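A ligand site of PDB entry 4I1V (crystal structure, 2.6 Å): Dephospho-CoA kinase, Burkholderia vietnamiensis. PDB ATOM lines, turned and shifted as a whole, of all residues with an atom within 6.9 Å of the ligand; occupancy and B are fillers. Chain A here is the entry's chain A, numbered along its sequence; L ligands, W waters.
The backbone NH (N) of Thr 187 lies within hydrogen-bond range of a nitrogen (N4) of the ligand (3.5 Å). N of Thr 24 is in hydrogen-bond range of O4 of the ligand (3.0 Å). A nitrogen (N3) of the ligand sits close to the backbone carbonyl oxygen (O) of Thr 187, 3.3 Å away. The backbone NH (N) of Gly 21 is in hydrogen-bond range of an oxygen (O6) of the ligand. An oxygen (O2) of the ligand lies within hydrogen-bond range of the backbone NH (N) of Lys 22 (3.1 Å). The side-chain hydroxyl of Thr 23 sits at hydrogen-bond distance from an oxygen (O1) of the ligand, at 2.7 Å. The backbone NH (N) of Gly 19 is in hydrogen-bond range of an oxygen (O3) of the ligand. An oxygen (O2) of the ligand lies within salt-bridge range of the side-chain amino group (NZ) of Lys 22. A nitrogen (N3) of the ligand lies within hydrogen-bond range of the side-chain amide oxygen (OD1) of Asn 183, at 2.8 Å. The side-chain hydroxyl (OG1) of Thr 24 is in hydrogen-bond range of an oxygen (O4) of the ligand, 2.4 Å away. The backbone NH of Thr 23 is in hydrogen-bond range of an oxygen (O1) of the ligand, at 3.0 Å. The backbone carbonyl oxygen (O) of Ala 185 sits at hydrogen-bond distance from a nitrogen (N3) of the ligand, 3.3 Å away.
OG of Ser 20 sits at hydrogen-bond distance from O of Gly 17, at 2.8 Å. OG of Ser 20 is in hydrogen-bond range of O of Val 138 (3.3 Å). NH1 of Arg 148 lies within hydrogen-bond range of O of Ser 20, at 3.0 Å. The side-chain amino group (NZ) of Lys 22 lies within hydrogen-bond range of the backbone carbonyl oxygen (O) of Gly 16 (2.8 Å). NH2 of Arg 148 lies within hydrogen-bond range of O of Asn 183 (2.8 Å). The backbone carbonyl oxygen (O) of Gly 19 is in hydrogen-bond range of the guanidinium group (NH1) of Arg 148, 2.9 Å away. The backbone carbonyl oxygen of Ser 20 is in hydrogen-bond range of the side-chain amide nitrogen of Asn 183, 2.9 Å away. The side-chain amino group (NZ) of Lys 22 sits at hydrogen-bond distance from the backbone carbonyl oxygen (O) of Gly 17 (2.9 Å).
A nitrogen (N4) of the ligand lies close to the backbone carbonyl oxygen (O) of Ala 186. A nitrogen (N3) of the ligand sits close to the backbone nitrogen (N) of Pro 188, 3.4 Å away. Residues that only touch the ligand: Arg 148, Ser 20, Gly 17 and Arg 152. Hydrophobic or aromatic side chains that line the ligand: Pro 188. The nearest printed residue that does not touch the ligand is Ile 18 (4.4 Å).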
ATOM      1  N   THR A  15       9.293  20.682  25.841  1.00  0.00           N
ATOM      2  CA  THR A  15      10.484  20.350  26.583  1.00  0.00           C
ATOM      3  C   THR A  15      11.691  20.210  25.638  1.00  0.00           C
ATOM      4  O   THR A  15      11.593  20.456  24.434  1.00  0.00           O
ATOM      5  CB  THR A  15      10.251  19.074  27.414  1.00  0.00           C
ATOM      6  OG1 THR A  15      11.332  18.925  28.338  1.00  0.00           O
ATOM      7  CG2 THR A  15      10.178  17.868  26.533  1.00  0.00           C
ATOM      8  N   GLY A  16      12.822  19.828  26.226  1.00  0.00           N
ATOM      9  CA  GLY A  16      14.082  19.782  25.515  1.00  0.00           C
ATOM     10  C   GLY A  16      15.230  20.027  26.481  1.00  0.00           C
ATOM     11  O   GLY A  16      15.069  20.739  27.440  1.00  0.00           O
ATOM     12  N   GLY A  17      16.397  19.464  26.187  1.00  0.00           N
ATOM     13  CA  GLY A  17      17.583  19.605  27.007  1.00  0.00           C
ATOM     14  C   GLY A  17      18.086  21.031  27.033  1.00  0.00           C
ATOM     15  O   GLY A  17      17.584  21.912  26.344  1.00  0.00           O
ATOM     16  N   ILE A  18      19.137  21.251  27.837  1.00  0.00           N
ATOM     17  CA  ILE A  18      19.688  22.581  27.977  1.00  0.00           C
ATOM     18  C   ILE A  18      20.289  23.018  26.647  1.00  0.00           C
ATOM     19  O   ILE A  18      21.049  22.288  26.021  1.00  0.00           O
ATOM     20  CB  ILE A  18      20.708  22.678  29.151  1.00  0.00           C
ATOM     21  CG1 ILE A  18      21.062  24.143  29.417  1.00  0.00           C
ATOM     22  CG2 ILE A  18      21.973  21.855  28.885  1.00  0.00           C
ATOM     23  CD1 ILE A  18      22.043  24.347  30.558  1.00  0.00           C
ATOM     24  N   GLY A  19      19.919  24.219  26.236  1.00  0.00           N
ATOM     25  CA  GLY A  19      20.465  24.821  25.016  1.00  0.00           C
ATOM     26  C   GLY A  19      19.839  24.328  23.725  1.00  0.00           C
ATOM     27  O   GLY A  19      20.332  24.660  22.659  1.00  0.00           O
ATOM     28  N   SER A  20      18.764  23.527  23.821  1.00  0.00           N
ATOM     29  CA  SER A  20      18.183  22.897  22.649  1.00  0.00           C
ATOM     30  C   SER A  20      17.323  23.835  21.861  1.00  0.00           C
ATOM     31  O   SER A  20      17.210  23.707  20.666  1.00  0.00           O
ATOM     32  CB  SER A  20      17.402  21.633  23.040  1.00  0.00           C
ATOM     33  OG  SER A  20      16.304  21.938  23.889  1.00  0.00           O
ATOM     34  N   GLY A  21      16.699  24.809  22.520  1.00  0.00           N
ATOM     35  CA  GLY A  21      15.897  25.808  21.828  1.00  0.00           C
ATOM     36  C   GLY A  21      14.483  26.010  22.323  1.00  0.00           C
ATOM     37  O   GLY A  21      13.667  26.623  21.623  1.00  0.00           O
ATOM     38  N   LYS A  22      14.187  25.553  23.531  1.00  0.00           N
ATOM     39  CA  LYS A  22      12.842  25.725  24.091  1.00  0.00           C
ATOM     40  C   LYS A  22      12.392  27.194  24.013  1.00  0.00           C
ATOM     41  O   LYS A  22      11.346  27.501  23.436  1.00  0.00           O
ATOM     42  CB  LYS A  22      12.808  25.256  25.524  1.00  0.00           C
ATOM     43  CG  LYS A  22      13.133  23.777  25.667  1.00  0.00           C
ATOM     44  CD  LYS A  22      13.068  23.308  27.110  1.00  0.00           C
ATOM     45  CE  LYS A  22      14.139  23.960  27.973  1.00  0.00           C
ATOM     46  NZ  LYS A  22      15.506  23.538  27.543  1.00  0.00           N
ATOM     47  N   THR A  23      13.197  28.099  24.530  1.00  0.00           N
ATOM     48  CA  THR A  23      12.815  29.491  24.514  1.00  0.00           C
ATOM     49  C   THR A  23      12.566  29.969  23.074  1.00  0.00           C
ATOM     50  O   THR A  23      11.565  30.636  22.778  1.00  0.00           O
ATOM     51  CB  THR A  23      13.906  30.365  25.157  1.00  0.00           C
ATOM     52  OG1 THR A  23      14.210  29.863  26.479  1.00  0.00           O
ATOM     53  CG2 THR A  23      13.458  31.807  25.226  1.00  0.00           C
ATOM     54  N   THR A  24      13.470  29.606  22.185  1.00  0.00           N
ATOM     55  CA  THR A  24      13.368  30.039  20.812  1.00  0.00           C
ATOM     56  C   THR A  24      12.071  29.563  20.155  1.00  0.00           C
ATOM     57  O   THR A  24      11.371  30.325  19.498  1.00  0.00           O
ATOM     58  CB  THR A  24      14.626  29.562  20.028  1.00  0.00           C
ATOM     59  OG1 THR A  24      15.788  30.104  20.652  1.00  0.00           O
ATOM     60  CG2 THR A  24      14.556  30.034  18.601  1.00  0.00           C
ATOM     61  N   VAL A  25      11.750  28.306  20.375  1.00  0.00           N
ATOM     62  CA  VAL A  25      10.557  27.747  19.775  1.00  0.00           C
ATOM     63  C   VAL A  25       9.312  28.296  20.454  1.00  0.00           C
ATOM     64  O   VAL A  25       8.352  28.667  19.807  1.00  0.00           O
ATOM     65  CB  VAL A  25      10.590  26.223  19.837  1.00  0.00           C
ATOM     66  CG1 VAL A  25       9.261  25.629  19.410  1.00  0.00           C
ATOM     67  CG2 VAL A  25      11.696  25.715  18.931  1.00  0.00           C
ATOM     68  N   VAL A 118       6.150  25.367  29.257  1.00  0.00           N
ATOM     69  CA  VAL A 118       7.578  25.107  29.008  1.00  0.00           C
ATOM     70  C   VAL A 118       8.173  24.482  30.262  1.00  0.00           C
ATOM     71  O   VAL A 118       8.294  25.129  31.286  1.00  0.00           O
ATOM     72  CB  VAL A 118       8.336  26.407  28.702  1.00  0.00           C
ATOM     73  CG1 VAL A 118       9.754  26.093  28.267  1.00  0.00           C
ATOM     74  CG2 VAL A 118       7.597  27.193  27.633  1.00  0.00           C
ATOM     75  N   VAL A 138      11.871  19.754  21.617  1.00  0.00           N
ATOM     76  CA  VAL A 138      12.805  20.470  20.771  1.00  0.00           C
ATOM     77  C   VAL A 138      14.145  19.768  20.883  1.00  0.00           C
ATOM     78  O   VAL A 138      14.772  19.763  21.940  1.00  0.00           O
ATOM     79  CB  VAL A 138      12.965  21.905  21.215  1.00  0.00           C
ATOM     80  CG1 VAL A 138      13.887  22.650  20.270  1.00  0.00           C
ATOM     81  CG2 VAL A 138      11.606  22.577  21.251  1.00  0.00           C
ATOM     82  N   THR A 144      25.819  20.405  19.860  1.00  0.00           N
ATOM     83  CA  THR A 144      25.192  21.700  19.616  1.00  0.00           C
ATOM     84  C   THR A 144      24.681  22.298  20.937  1.00  0.00           C
ATOM     85  O   THR A 144      24.797  23.509  21.160  1.00  0.00           O
ATOM     86  CB  THR A 144      24.068  21.614  18.605  1.00  0.00           C
ATOM     87  OG1 THR A 144      24.566  21.020  17.395  1.00  0.00           O
ATOM     88  CG2 THR A 144      23.524  23.004  18.293  1.00  0.00           C
ATOM     89  N   ARG A 148      26.249  25.937  22.191  1.00  0.00           N
ATOM     90  CA  ARG A 148      25.342  27.025  22.422  1.00  0.00           C
ATOM     91  C   ARG A 148      25.414  27.505  23.836  1.00  0.00           C
ATOM     92  O   ARG A 148      25.306  28.707  24.068  1.00  0.00           O
ATOM     93  CB  ARG A 148      23.887  26.657  22.154  1.00  0.00           C
ATOM     94  CG  ARG A 148      23.508  26.666  20.690  1.00  0.00           C
ATOM     95  CD  ARG A 148      22.171  25.954  20.567  1.00  0.00           C
ATOM     96  NE  ARG A 148      21.784  25.771  19.186  1.00  0.00           N
ATOM     97  CZ  ARG A 148      20.696  25.131  18.831  1.00  0.00           C
ATOM     98  NH1 ARG A 148      19.902  24.601  19.743  1.00  0.00           N
ATOM     99  NH2 ARG A 148      20.404  25.008  17.548  1.00  0.00           N
ATOM    100  N   VAL A 149      25.526  26.575  24.783  1.00  0.00           N
ATOM    101  CA  VAL A 149      25.502  26.945  26.202  1.00  0.00           C
ATOM    102  C   VAL A 149      26.859  27.516  26.611  1.00  0.00           C
ATOM    103  O   VAL A 149      26.935  28.351  27.488  1.00  0.00           O
ATOM    104  CB  VAL A 149      25.107  25.754  27.086  1.00  0.00           C
ATOM    105  CG1 VAL A 149      25.279  26.087  28.556  1.00  0.00           C
ATOM    106  CG2 VAL A 149      23.671  25.360  26.803  1.00  0.00           C
ATOM    107  N   GLN A 151      28.723  29.370  24.493  1.00  0.00           N
ATOM    108  CA  GLN A 151      28.558  30.704  23.914  1.00  0.00           C
ATOM    109  C   GLN A 151      27.676  31.597  24.762  1.00  0.00           C
ATOM    110  O   GLN A 151      28.045  32.707  25.088  1.00  0.00           O
ATOM    111  CB  GLN A 151      27.929  30.580  22.514  1.00  0.00           C
ATOM    112  CG  GLN A 151      27.662  31.885  21.788  1.00  0.00           C
ATOM    113  CD  GLN A 151      28.927  32.644  21.467  1.00  0.00           C
ATOM    114  OE1 GLN A 151      29.926  32.036  21.049  1.00  0.00           O
ATOM    115  NE2 GLN A 151      28.905  33.958  21.668  1.00  0.00           N
ATOM    116  N   ARG A 152      26.486  31.123  25.094  1.00  0.00           N
ATOM    117  CA  ARG A 152      25.477  32.012  25.650  1.00  0.00           C
ATOM    118  C   ARG A 152      25.541  32.149  27.176  1.00  0.00           C
ATOM    119  O   ARG A 152      24.939  33.058  27.698  1.00  0.00           O
ATOM    120  CB  ARG A 152      24.077  31.607  25.174  1.00  0.00           C
ATOM    121  N   ASN A 153      26.233  31.255  27.897  1.00  0.00           N
ATOM    122  CA  ASN A 153      26.467  31.457  29.331  1.00  0.00           C
ATOM    123  C   ASN A 153      27.921  31.451  29.797  1.00  0.00           C
ATOM    124  O   ASN A 153      28.199  31.722  30.965  1.00  0.00           O
ATOM    125  CB  ASN A 153      25.671  30.420  30.128  1.00  0.00           C
ATOM    126  CG  ASN A 153      24.170  30.533  29.893  1.00  0.00           C
ATOM    127  OD1 ASN A 153      23.481  31.204  30.656  1.00  0.00           O
ATOM    128  ND2 ASN A 153      23.678  29.929  28.819  1.00  0.00           N
ATOM    129  N   ASN A 183      16.154  21.243  16.122  1.00  0.00           N
ATOM    130  CA  ASN A 183      16.649  22.598  16.013  1.00  0.00           C
ATOM    131  C   ASN A 183      18.150  22.527  15.951  1.00  0.00           C
ATOM    132  O   ASN A 183      18.799  22.734  16.959  1.00  0.00           O
ATOM    133  CB  ASN A 183      16.202  23.429  17.233  1.00  0.00           C
ATOM    134  CG  ASN A 183      16.788  24.833  17.230  1.00  0.00           C
ATOM    135  OD1 ASN A 183      17.091  25.385  16.188  1.00  0.00           O
ATOM    136  ND2 ASN A 183      16.928  25.413  18.394  1.00  0.00           N
ATOM    137  N   ASP A 184      18.684  22.197  14.779  1.00  0.00           N
ATOM    138  CA  ASP A 184      20.153  22.071  14.605  1.00  0.00           C
ATOM    139  C   ASP A 184      20.705  22.837  13.399  1.00  0.00           C
ATOM    140  O   ASP A 184      21.823  22.594  12.996  1.00  0.00           O
ATOM    141  CB  ASP A 184      20.620  20.608  14.529  1.00  0.00           C
ATOM    142  CG  ASP A 184      22.158  20.468  14.623  1.00  0.00           C
ATOM    143  OD1 ASP A 184      22.807  21.062  15.560  1.00  0.00           O
ATOM    144  OD2 ASP A 184      22.719  19.749  13.751  1.00  0.00           O
ATOM    145  N   ALA A 185      19.964  23.749  12.801  1.00  0.00           N
ATOM    146  CA  ALA A 185      20.525  24.521  11.704  1.00  0.00           C
ATOM    147  C   ALA A 185      21.428  25.590  12.302  1.00  0.00           C
ATOM    148  O   ALA A 185      21.322  25.890  13.505  1.00  0.00           O
ATOM    149  CB  ALA A 185      19.414  25.130  10.866  1.00  0.00           C
ATOM    150  N   ALA A 186      22.315  26.132  11.486  1.00  0.00           N
ATOM    151  CA  ALA A 186      23.135  27.285  11.876  1.00  0.00           C
ATOM    152  C   ALA A 186      22.276  28.467  12.365  1.00  0.00           C
ATOM    153  O   ALA A 186      22.728  29.322  13.144  1.00  0.00           O
ATOM    154  CB  ALA A 186      24.027  27.732  10.717  1.00  0.00           C
ATOM    155  N   THR A 187      21.012  28.448  11.915  1.00  0.00           N
ATOM    156  CA  THR A 187      20.090  29.548  12.046  1.00  0.00           C
ATOM    157  C   THR A 187      18.675  29.019  12.385  1.00  0.00           C
ATOM    158  O   THR A 187      18.307  27.889  11.961  1.00  0.00           O
ATOM    159  CB  THR A 187      20.140  30.375  10.731  1.00  0.00           C
ATOM    160  OG1 THR A 187      20.987  31.513  10.932  1.00  0.00           O
ATOM    161  CG2 THR A 187      18.775  30.840  10.257  1.00  0.00           C
ATOM    162  N   PRO A 188      17.898  29.807  13.155  1.00  0.00           N
ATOM    163  CA  PRO A 188      16.520  29.536  13.562  1.00  0.00           C
ATOM    164  C   PRO A 188      15.430  30.015  12.598  1.00  0.00           C
ATOM    165  O   PRO A 188      14.256  29.826  12.864  1.00  0.00           O
ATOM    166  CB  PRO A 188      16.402  30.288  14.897  1.00  0.00           C
ATOM    167  CG  PRO A 188      17.370  31.409  14.801  1.00  0.00           C
ATOM    168  CD  PRO A 188      18.478  30.948  13.897  1.00  0.00           C
ATOM    169  N   ASP A 189      15.807  30.599  11.473  1.00  0.00           N
ATOM    170  CA  ASP A 189      14.829  31.139  10.518  1.00  0.00           C
ATOM    171  C   ASP A 189      13.823  30.092   9.987  1.00  0.00           C
ATOM    172  O   ASP A 189      12.648  30.405   9.740  1.00  0.00           O
ATOM    173  CB  ASP A 189      15.563  31.812   9.342  1.00  0.00           C
ATOM    174  CG  ASP A 189      16.413  33.053   9.779  1.00  0.00           C
ATOM    175  OD1 ASP A 189      17.042  33.691   8.877  1.00  0.00           O
ATOM    176  OD2 ASP A 189      16.453  33.395  10.995  1.00  0.00           O
ATOM    177  N   LEU A 191      12.721  27.343  11.492  1.00  0.00           N
ATOM    178  CA  LEU A 191      11.835  26.846  12.526  1.00  0.00           C
ATOM    179  C   LEU A 191      10.399  27.324  12.354  1.00  0.00           C
ATOM    180  O   LEU A 191       9.465  26.575  12.644  1.00  0.00           O
ATOM    181  CB  LEU A 191      12.321  27.303  13.902  1.00  0.00           C
ATOM    182  CG  LEU A 191      13.674  26.746  14.345  1.00  0.00           C
ATOM    183  CD1 LEU A 191      13.997  27.277  15.720  1.00  0.00           C
ATOM    184  CD2 LEU A 191      13.670  25.223  14.367  1.00  0.00           C
HETATM  185  P1  LIG L   1      16.731  26.641  25.797  1.00  0.00           P
HETATM  186  O1  LIG L   1      15.618  27.600  26.167  1.00  0.00           O
HETATM  187  O2  LIG L   1      16.304  25.205  25.744  1.00  0.00           O
HETATM  188  O3  LIG L   1      18.055  26.847  26.498  1.00  0.00           O
HETATM  189  P2  LIG L   1      17.236  28.579  23.775  1.00  0.00           P
HETATM  190  O4  LIG L   1      16.320  28.732  22.578  1.00  0.00           O
HETATM  191  O5  LIG L   1      17.114  29.575  24.885  1.00  0.00           O
HETATM  192  O6  LIG L   1      17.176  27.058  24.311  1.00  0.00           O
HETATM  193  O7  LIG L   1      18.829  28.606  23.605  1.00  0.00           O
HETATM  194  C1  LIG L   1      19.726  28.150  22.623  1.00  0.00           C
HETATM  195  C2  LIG L   1      20.763  29.233  22.471  1.00  0.00           C
HETATM  196  O8  LIG L   1      21.278  29.168  21.132  1.00  0.00           O
HETATM  197  C3  LIG L   1      20.158  30.617  22.539  1.00  0.00           C
HETATM  198  O9  LIG L   1      21.169  31.576  22.772  1.00  0.00           O
HETATM  199  C4  LIG L   1      19.632  30.885  21.146  1.00  0.00           C
HETATM  200  O10 LIG L   1      19.702  32.272  20.840  1.00  0.00           O
HETATM  201  C5  LIG L   1      20.600  30.110  20.274  1.00  0.00           C
HETATM  202  N1  LIG L   1      19.928  29.330  19.238  1.00  0.00           N
HETATM  203  C6  LIG L   1      18.811  28.562  19.358  1.00  0.00           C
HETATM  204  N2  LIG L   1      18.506  27.961  18.190  1.00  0.00           N
HETATM  205  C7  LIG L   1      19.435  28.359  17.323  1.00  0.00           C
HETATM  206  C8  LIG L   1      19.693  28.102  15.904  1.00  0.00           C
HETATM  207  N3  LIG L   1      18.876  27.291  15.201  1.00  0.00           N
HETATM  208  N4  LIG L   1      20.779  28.704  15.367  1.00  0.00           N
HETATM  209  C9  LIG L   1      21.600  29.532  16.070  1.00  0.00           C
HETATM  210  N5  LIG L   1      21.402  29.816  17.357  1.00  0.00           N
HETATM  211  C10 LIG L   1      20.367  29.253  18.006  1.00  0.00           C
HETATM  212  O   HOH W   1      17.275  24.946  13.177  1.00  0.00           O
HETATM  213  O   HOH W   2      20.790  28.405  27.427  1.00  0.00           O
HETATM  214  O   HOH W   3      16.880  32.116  24.232  1.00  0.00           O
